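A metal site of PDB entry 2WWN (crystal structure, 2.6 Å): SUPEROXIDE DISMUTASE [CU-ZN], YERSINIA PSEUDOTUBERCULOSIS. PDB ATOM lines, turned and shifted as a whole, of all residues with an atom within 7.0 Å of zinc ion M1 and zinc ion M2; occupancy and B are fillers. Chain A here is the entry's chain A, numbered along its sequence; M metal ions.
Zinc ion M1 is bound by OD1 of Asp 108 (2.1 Å), ND1 of His 96 (2.3 Å), ND1 of His 87 (2.3 Å) and ND1 of His 105 (2.4 Å).
The side-chain carboxylate (OD2) of Asp 108 sits at hydrogen-bond distance from the backbone NH (N) of Gly 98 (2.9 Å). The backbone NH (N) of His 143 lies within hydrogen-bond range of the backbone carbonyl oxygen (O) of Gly 60, 3.1 Å away. A ring nitrogen (ND1) of His 143 lies within hydrogen-bond range of the backbone carbonyl oxygen (O) of Gly 160. OD1 of Asp 147 sits at hydrogen-bond distance from NE2 of His 96 (2.9 Å). ND1 of His 64 lies close to O of Gly 86 (3.3 Å). ND1 of His 64 is in hydrogen-bond range of O of Gly 85 (2.8 Å). NE2 of His 62 is in hydrogen-bond range of OD2 of Asp 147 (2.8 Å). The backbone NH of His 105 is in hydrogen-bond range of the backbone carbonyl oxygen of Val 95 (2.9 Å).
Four residues have an atom within 4 Å of zinc ion M2: His 62, His 64, His 87 and His 143.
Of the 29 residues printed, 4 come within 4 Å of zinc ion M1.
Zinc ion M2 is bound by a ring nitrogen (NE2) of His 87 (2.2 Å), a ring nitrogen (NE2) of His 143 (2.2 Å), a ring nitrogen (NE2) of His 64 (2.3 Å) and a ring nitrogen (ND1) of His 62 (2.3 Å). Zinc ion M2 has four donor atoms within binding distance.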
ATOM      1  N   GLY A  60      -6.546  -7.289  30.528  1.00  0.00           N
ATOM      2  CA  GLY A  60      -6.398  -5.884  30.225  1.00  0.00           C
ATOM      3  C   GLY A  60      -5.564  -5.731  28.968  1.00  0.00           C
ATOM      4  O   GLY A  60      -4.532  -6.397  28.802  1.00  0.00           O
ATOM      5  N   PHE A  61      -6.000  -4.838  28.078  1.00  0.00           N
ATOM      6  CA  PHE A  61      -5.415  -4.731  26.752  1.00  0.00           C
ATOM      7  C   PHE A  61      -5.396  -3.262  26.353  1.00  0.00           C
ATOM      8  O   PHE A  61      -6.395  -2.735  25.858  1.00  0.00           O
ATOM      9  CB  PHE A  61      -6.262  -5.556  25.776  1.00  0.00           C
ATOM     10  CG  PHE A  61      -5.602  -5.808  24.439  1.00  0.00           C
ATOM     11  CD1 PHE A  61      -4.248  -6.092  24.356  1.00  0.00           C
ATOM     12  CD2 PHE A  61      -6.363  -5.799  23.266  1.00  0.00           C
ATOM     13  CE1 PHE A  61      -3.651  -6.345  23.138  1.00  0.00           C
ATOM     14  CE2 PHE A  61      -5.777  -6.050  22.048  1.00  0.00           C
ATOM     15  CZ  PHE A  61      -4.421  -6.323  21.975  1.00  0.00           C
ATOM     16  N   HIS A  62      -4.272  -2.591  26.581  1.00  0.00           N
ATOM     17  CA  HIS A  62      -4.221  -1.139  26.415  1.00  0.00           C
ATOM     18  C   HIS A  62      -3.015  -0.677  25.588  1.00  0.00           C
ATOM     19  O   HIS A  62      -2.031  -1.393  25.455  1.00  0.00           O
ATOM     20  CB  HIS A  62      -4.184  -0.448  27.784  1.00  0.00           C
ATOM     21  CG  HIS A  62      -4.962  -1.174  28.848  1.00  0.00           C
ATOM     22  ND1 HIS A  62      -4.352  -1.765  29.935  1.00  0.00           N
ATOM     23  CD2 HIS A  62      -6.287  -1.398  28.992  1.00  0.00           C
ATOM     24  CE1 HIS A  62      -5.278  -2.318  30.702  1.00  0.00           C
ATOM     25  NE2 HIS A  62      -6.458  -2.112  30.151  1.00  0.00           N
ATOM     26  N   LEU A  63      -3.114   0.535  25.038  1.00  0.00           N
ATOM     27  CA  LEU A  63      -1.973   1.186  24.405  1.00  0.00           C
ATOM     28  C   LEU A  63      -1.297   2.092  25.413  1.00  0.00           C
ATOM     29  O   LEU A  63      -1.951   2.918  26.052  1.00  0.00           O
ATOM     30  CB  LEU A  63      -2.411   2.015  23.200  1.00  0.00           C
ATOM     31  CG  LEU A  63      -2.898   1.254  21.972  1.00  0.00           C
ATOM     32  CD1 LEU A  63      -3.618   2.200  21.035  1.00  0.00           C
ATOM     33  CD2 LEU A  63      -1.736   0.556  21.268  1.00  0.00           C
ATOM     34  N   HIS A  64       0.012   1.936  25.570  1.00  0.00           N
ATOM     35  CA  HIS A  64       0.761   2.773  26.494  1.00  0.00           C
ATOM     36  C   HIS A  64       1.546   3.847  25.734  1.00  0.00           C
ATOM     37  O   HIS A  64       1.814   3.699  24.534  1.00  0.00           O
ATOM     38  CB  HIS A  64       1.658   1.917  27.385  1.00  0.00           C
ATOM     39  CG  HIS A  64       0.900   1.123  28.404  1.00  0.00           C
ATOM     40  ND1 HIS A  64       1.209   1.160  29.749  1.00  0.00           N
ATOM     41  CD2 HIS A  64      -0.169   0.299  28.279  1.00  0.00           C
ATOM     42  CE1 HIS A  64       0.370   0.371  30.406  1.00  0.00           C
ATOM     43  NE2 HIS A  64      -0.474  -0.162  29.537  1.00  0.00           N
ATOM     44  N   GLY A  85       5.578   3.466  29.991  1.00  0.00           N
ATOM     45  CA  GLY A  85       4.811   4.532  30.619  1.00  0.00           C
ATOM     46  C   GLY A  85       3.389   4.103  30.920  1.00  0.00           C
ATOM     47  O   GLY A  85       3.080   2.910  30.882  1.00  0.00           O
ATOM     48  N   GLY A  86       2.531   5.067  31.234  1.00  0.00           N
ATOM     49  CA  GLY A  86       1.143   4.785  31.533  1.00  0.00           C
ATOM     50  C   GLY A  86       0.325   4.613  30.274  1.00  0.00           C
ATOM     51  O   GLY A  86       0.890   4.437  29.180  1.00  0.00           O
ATOM     52  N   HIS A  87      -0.995   4.673  30.405  1.00  0.00           N
ATOM     53  CA  HIS A  87      -1.889   4.552  29.252  1.00  0.00           C
ATOM     54  C   HIS A  87      -1.894   5.793  28.369  1.00  0.00           C
ATOM     55  O   HIS A  87      -1.818   6.927  28.861  1.00  0.00           O
ATOM     56  CB  HIS A  87      -3.319   4.216  29.695  1.00  0.00           C
ATOM     57  CG  HIS A  87      -3.454   2.889  30.362  1.00  0.00           C
ATOM     58  ND1 HIS A  87      -4.460   2.613  31.267  1.00  0.00           N
ATOM     59  CD2 HIS A  87      -2.719   1.758  30.271  1.00  0.00           C
ATOM     60  CE1 HIS A  87      -4.332   1.377  31.699  1.00  0.00           C
ATOM     61  NE2 HIS A  87      -3.291   0.829  31.112  1.00  0.00           N
ATOM     62  N   LEU A  88      -1.989   5.573  27.052  1.00  0.00           N
ATOM     63  CA  LEU A  88      -2.111   6.643  26.081  1.00  0.00           C
ATOM     64  C   LEU A  88      -3.293   7.551  26.437  1.00  0.00           C
ATOM     65  O   LEU A  88      -4.439   7.097  26.471  1.00  0.00           O
ATOM     66  CB  LEU A  88      -2.283   6.052  24.682  1.00  0.00           C
ATOM     67  CG  LEU A  88      -2.390   6.991  23.482  1.00  0.00           C
ATOM     68  CD1 LEU A  88      -1.112   7.807  23.289  1.00  0.00           C
ATOM     69  CD2 LEU A  88      -2.712   6.182  22.229  1.00  0.00           C
ATOM     70  N   VAL A  95      -7.796   9.275  33.614  1.00  0.00           N
ATOM     71  CA  VAL A  95      -8.762   8.301  34.123  1.00  0.00           C
ATOM     72  C   VAL A  95      -8.949   7.109  33.184  1.00  0.00           C
ATOM     73  O   VAL A  95      -8.859   7.242  31.960  1.00  0.00           O
ATOM     74  CB  VAL A  95     -10.120   8.981  34.445  1.00  0.00           C
ATOM     75  CG1 VAL A  95     -10.813   9.407  33.160  1.00  0.00           C
ATOM     76  CG2 VAL A  95     -10.994   8.058  35.263  1.00  0.00           C
ATOM     77  N   HIS A  96      -9.209   5.937  33.767  1.00  0.00           N
ATOM     78  CA  HIS A  96      -9.405   4.709  32.991  1.00  0.00           C
ATOM     79  C   HIS A  96     -10.902   4.380  32.862  1.00  0.00           C
ATOM     80  O   HIS A  96     -11.567   4.036  33.855  1.00  0.00           O
ATOM     81  CB  HIS A  96      -8.640   3.561  33.644  1.00  0.00           C
ATOM     82  CG  HIS A  96      -8.718   2.256  32.906  1.00  0.00           C
ATOM     83  ND1 HIS A  96      -7.810   1.892  31.931  1.00  0.00           N
ATOM     84  CD2 HIS A  96      -9.592   1.226  33.009  1.00  0.00           C
ATOM     85  CE1 HIS A  96      -8.130   0.697  31.462  1.00  0.00           C
ATOM     86  NE2 HIS A  96      -9.205   0.269  32.097  1.00  0.00           N
ATOM     87  N   LEU A  97     -11.433   4.490  31.643  1.00  0.00           N
ATOM     88  CA  LEU A  97     -12.873   4.318  31.431  1.00  0.00           C
ATOM     89  C   LEU A  97     -13.244   3.401  30.257  1.00  0.00           C
ATOM     90  O   LEU A  97     -14.420   3.277  29.903  1.00  0.00           O
ATOM     91  CB  LEU A  97     -13.578   5.670  31.304  1.00  0.00           C
ATOM     92  CG  LEU A  97     -13.701   6.435  32.636  1.00  0.00           C
ATOM     93  CD1 LEU A  97     -14.179   7.867  32.435  1.00  0.00           C
ATOM     94  CD2 LEU A  97     -14.614   5.671  33.591  1.00  0.00           C
ATOM     95  N   GLY A  98     -12.260   2.748  29.648  1.00  0.00           N
ATOM     96  CA  GLY A  98     -12.526   1.747  28.642  1.00  0.00           C
ATOM     97  C   GLY A  98     -12.665   2.256  27.215  1.00  0.00           C
ATOM     98  O   GLY A  98     -12.572   3.450  26.959  1.00  0.00           O
ATOM     99  N   GLY A 104     -12.197   8.897  29.163  1.00  0.00           N
ATOM    100  CA  GLY A 104     -11.028   8.233  29.690  1.00  0.00           C
ATOM    101  C   GLY A 104      -9.890   8.114  28.689  1.00  0.00           C
ATOM    102  O   GLY A 104      -9.945   8.687  27.598  1.00  0.00           O
ATOM    103  N   HIS A 105      -8.863   7.361  29.081  1.00  0.00           N
ATOM    104  CA  HIS A 105      -7.675   7.136  28.259  1.00  0.00           C
ATOM    105  C   HIS A 105      -8.000   6.660  26.839  1.00  0.00           C
ATOM    106  O   HIS A 105      -8.598   5.602  26.637  1.00  0.00           O
ATOM    107  CB  HIS A 105      -6.774   6.079  28.916  1.00  0.00           C
ATOM    108  CG  HIS A 105      -6.303   6.437  30.287  1.00  0.00           C
ATOM    109  ND1 HIS A 105      -6.190   5.514  31.306  1.00  0.00           N
ATOM    110  CD2 HIS A 105      -5.895   7.622  30.808  1.00  0.00           C
ATOM    111  CE1 HIS A 105      -5.747   6.108  32.396  1.00  0.00           C
ATOM    112  NE2 HIS A 105      -5.558   7.387  32.124  1.00  0.00           N
ATOM    113  N   LEU A 106      -7.552   7.424  25.840  1.00  0.00           N
ATOM    114  CA  LEU A 106      -7.716   7.015  24.446  1.00  0.00           C
ATOM    115  C   LEU A 106      -7.109   5.627  24.183  1.00  0.00           C
ATOM    116  O   LEU A 106      -7.545   4.914  23.273  1.00  0.00           O
ATOM    117  CB  LEU A 106      -7.078   8.027  23.499  1.00  0.00           C
ATOM    118  CG  LEU A 106      -7.139   7.674  22.001  1.00  0.00           C
ATOM    119  CD1 LEU A 106      -8.574   7.621  21.509  1.00  0.00           C
ATOM    120  CD2 LEU A 106      -6.326   8.657  21.168  1.00  0.00           C
ATOM    121  N   GLY A 107      -6.113   5.256  24.976  1.00  0.00           N
ATOM    122  CA  GLY A 107      -5.417   3.993  24.795  1.00  0.00           C
ATOM    123  C   GLY A 107      -6.158   2.782  25.326  1.00  0.00           C
ATOM    124  O   GLY A 107      -5.603   1.679  25.340  1.00  0.00           O
ATOM    125  N   ASP A 108      -7.394   2.974  25.768  1.00  0.00           N
ATOM    126  CA  ASP A 108      -8.195   1.898  26.338  1.00  0.00           C
ATOM    127  C   ASP A 108      -8.863   1.037  25.267  1.00  0.00           C
ATOM    128  O   ASP A 108      -9.744   1.506  24.537  1.00  0.00           O
ATOM    129  CB  ASP A 108      -9.264   2.448  27.276  1.00  0.00           C
ATOM    130  CG  ASP A 108      -8.679   2.944  28.576  1.00  0.00           C
ATOM    131  OD1 ASP A 108      -7.445   2.832  28.749  1.00  0.00           O
ATOM    132  OD2 ASP A 108      -9.443   3.429  29.442  1.00  0.00           O
ATOM    133  N   LEU A 109      -8.443  -0.225  25.192  1.00  0.00           N
ATOM    134  CA  LEU A 109      -9.048  -1.175  24.279  1.00  0.00           C
ATOM    135  C   LEU A 109      -9.929  -2.152  25.051  1.00  0.00           C
ATOM    136  O   LEU A 109      -9.866  -2.207  26.280  1.00  0.00           O
ATOM    137  CB  LEU A 109      -7.961  -1.909  23.497  1.00  0.00           C
ATOM    138  CG  LEU A 109      -6.817  -1.024  22.997  1.00  0.00           C
ATOM    139  CD1 LEU A 109      -5.727  -1.850  22.332  1.00  0.00           C
ATOM    140  CD2 LEU A 109      -7.330   0.072  22.070  1.00  0.00           C
ATOM    141  N   MET A 141      -0.059  -3.385  25.065  1.00  0.00           N
ATOM    142  CA  MET A 141       0.233  -4.043  26.335  1.00  0.00           C
ATOM    143  C   MET A 141      -0.795  -5.107  26.721  1.00  0.00           C
ATOM    144  O   MET A 141      -1.998  -4.931  26.513  1.00  0.00           O
ATOM    145  CB  MET A 141       0.321  -3.003  27.456  1.00  0.00           C
ATOM    146  CG  MET A 141       0.969  -3.514  28.729  1.00  0.00           C
ATOM    147  SD  MET A 141       2.773  -3.588  28.623  1.00  0.00           S
ATOM    148  CE  MET A 141       3.154  -1.845  28.437  1.00  0.00           C
ATOM    149  N   ILE A 142      -0.304  -6.206  27.306  1.00  0.00           N
ATOM    150  CA  ILE A 142      -1.165  -7.291  27.776  1.00  0.00           C
ATOM    151  C   ILE A 142      -0.912  -7.580  29.257  1.00  0.00           C
ATOM    152  O   ILE A 142       0.205  -7.890  29.655  1.00  0.00           O
ATOM    153  CB  ILE A 142      -0.964  -8.577  26.949  1.00  0.00           C
ATOM    154  CG1 ILE A 142      -1.241  -8.304  25.469  1.00  0.00           C
ATOM    155  CG2 ILE A 142      -1.870  -9.681  27.469  1.00  0.00           C
ATOM    156  CD1 ILE A 142      -1.001  -9.480  24.573  1.00  0.00           C
ATOM    157  N   HIS A 143      -1.966  -7.470  30.059  1.00  0.00           N
ATOM    158  CA  HIS A 143      -1.835  -7.579  31.514  1.00  0.00           C
ATOM    159  C   HIS A 143      -2.139  -8.972  32.045  1.00  0.00           C
ATOM    160  O   HIS A 143      -2.682  -9.825  31.335  1.00  0.00           O
ATOM    161  CB  HIS A 143      -2.722  -6.549  32.214  1.00  0.00           C
ATOM    162  CG  HIS A 143      -2.243  -5.145  32.056  1.00  0.00           C
ATOM    163  ND1 HIS A 143      -1.379  -4.542  32.960  1.00  0.00           N
ATOM    164  CD2 HIS A 143      -2.498  -4.214  31.106  1.00  0.00           C
ATOM    165  CE1 HIS A 143      -1.133  -3.302  32.572  1.00  0.00           C
ATOM    166  NE2 HIS A 143      -1.801  -3.080  31.453  1.00  0.00           N
ATOM    167  N   ASP A 147      -9.980  -6.432  32.880  1.00  0.00           N
ATOM    168  CA  ASP A 147     -10.310  -5.019  32.742  1.00  0.00           C
ATOM    169  C   ASP A 147     -11.814  -4.781  32.838  1.00  0.00           C
ATOM    170  O   ASP A 147     -12.580  -5.263  32.005  1.00  0.00           O
ATOM    171  CB  ASP A 147      -9.783  -4.446  31.418  1.00  0.00           C
ATOM    172  CG  ASP A 147      -9.815  -2.920  31.385  1.00  0.00           C
ATOM    173  OD1 ASP A 147     -10.411  -2.325  32.314  1.00  0.00           O
ATOM    174  OD2 ASP A 147      -9.254  -2.333  30.440  1.00  0.00           O
ATOM    175  N   ASP A 151     -11.676   2.696  37.243  1.00  0.00           N
ATOM    176  CA  ASP A 151     -10.643   2.784  38.270  1.00  0.00           C
ATOM    177  C   ASP A 151     -11.106   2.170  39.589  1.00  0.00           C
ATOM    178  O   ASP A 151     -10.354   2.136  40.563  1.00  0.00           O
ATOM    179  CB  ASP A 151     -10.205   4.243  38.468  1.00  0.00           C
ATOM    180  CG  ASP A 151      -9.393   4.783  37.300  1.00  0.00           C
ATOM    181  OD1 ASP A 151      -8.579   4.020  36.748  1.00  0.00           O
ATOM    182  OD2 ASP A 151      -9.571   5.971  36.931  1.00  0.00           O
ATOM    183  N   LEU A 156      -6.918   1.302  36.955  1.00  0.00           N
ATOM    184  CA  LEU A 156      -6.652   0.857  35.589  1.00  0.00           C
ATOM    185  C   LEU A 156      -7.311  -0.476  35.258  1.00  0.00           C
ATOM    186  O   LEU A 156      -6.703  -1.334  34.621  1.00  0.00           O
ATOM    187  CB  LEU A 156      -5.150   0.781  35.350  1.00  0.00           C
ATOM    188  CG  LEU A 156      -4.411   2.097  35.633  1.00  0.00           C
ATOM    189  CD1 LEU A 156      -2.902   1.904  35.605  1.00  0.00           C
ATOM    190  CD2 LEU A 156      -4.846   3.176  34.659  1.00  0.00           C
ATOM    191  N   GLY A 157      -8.564  -0.647  35.700  1.00  0.00           N
ATOM    192  CA  GLY A 157      -9.357  -1.807  35.343  1.00  0.00           C
ATOM    193  C   GLY A 157      -8.959  -3.097  36.023  1.00  0.00           C
ATOM    194  O   GLY A 157      -9.575  -4.143  35.810  1.00  0.00           O
ATOM    195  N   GLY A 159      -5.896  -4.395  35.709  1.00  0.00           N
ATOM    196  CA  GLY A 159      -4.948  -5.061  34.850  1.00  0.00           C
ATOM    197  C   GLY A 159      -3.756  -5.607  35.619  1.00  0.00           C
ATOM    198  O   GLY A 159      -3.288  -6.720  35.342  1.00  0.00           O
ATOM    199  N   GLY A 160      -3.272  -4.837  36.585  1.00  0.00           N
ATOM    200  CA  GLY A 160      -2.128  -5.231  37.382  1.00  0.00           C
ATOM    201  C   GLY A 160      -0.861  -5.346  36.562  1.00  0.00           C
ATOM    202  O   GLY A 160      -0.576  -4.504  35.715  1.00  0.00           O
ATOM    203  N   ARG A 162       2.237  -6.174  34.033  1.00  0.00           N
ATOM    204  CA  ARG A 162       2.372  -6.238  32.585  1.00  0.00           C
ATOM    205  C   ARG A 162       3.053  -7.553  32.237  1.00  0.00           C
ATOM    206  O   ARG A 162       4.143  -7.832  32.712  1.00  0.00           O
ATOM    207  CB  ARG A 162       3.192  -5.038  32.076  1.00  0.00           C
ATOM    208  CG  ARG A 162       2.727  -3.728  32.677  1.00  0.00           C
ATOM    209  CD  ARG A 162       3.449  -2.504  32.145  1.00  0.00           C
ATOM    210  NE  ARG A 162       2.958  -1.287  32.804  1.00  0.00           N
ATOM    211  CZ  ARG A 162       3.303  -0.047  32.477  1.00  0.00           C
ATOM    212  NH1 ARG A 162       4.142   0.176  31.475  1.00  0.00           N
ATOM    213  NH2 ARG A 162       2.791   0.972  33.152  1.00  0.00           N
HETATM  214 ZN    ZN M   1      -6.597   3.292  30.637  1.00  0.00          ZN
HETATM  215 ZN    ZN M   2      -2.243  -1.058  30.693  1.00  0.00          ZN
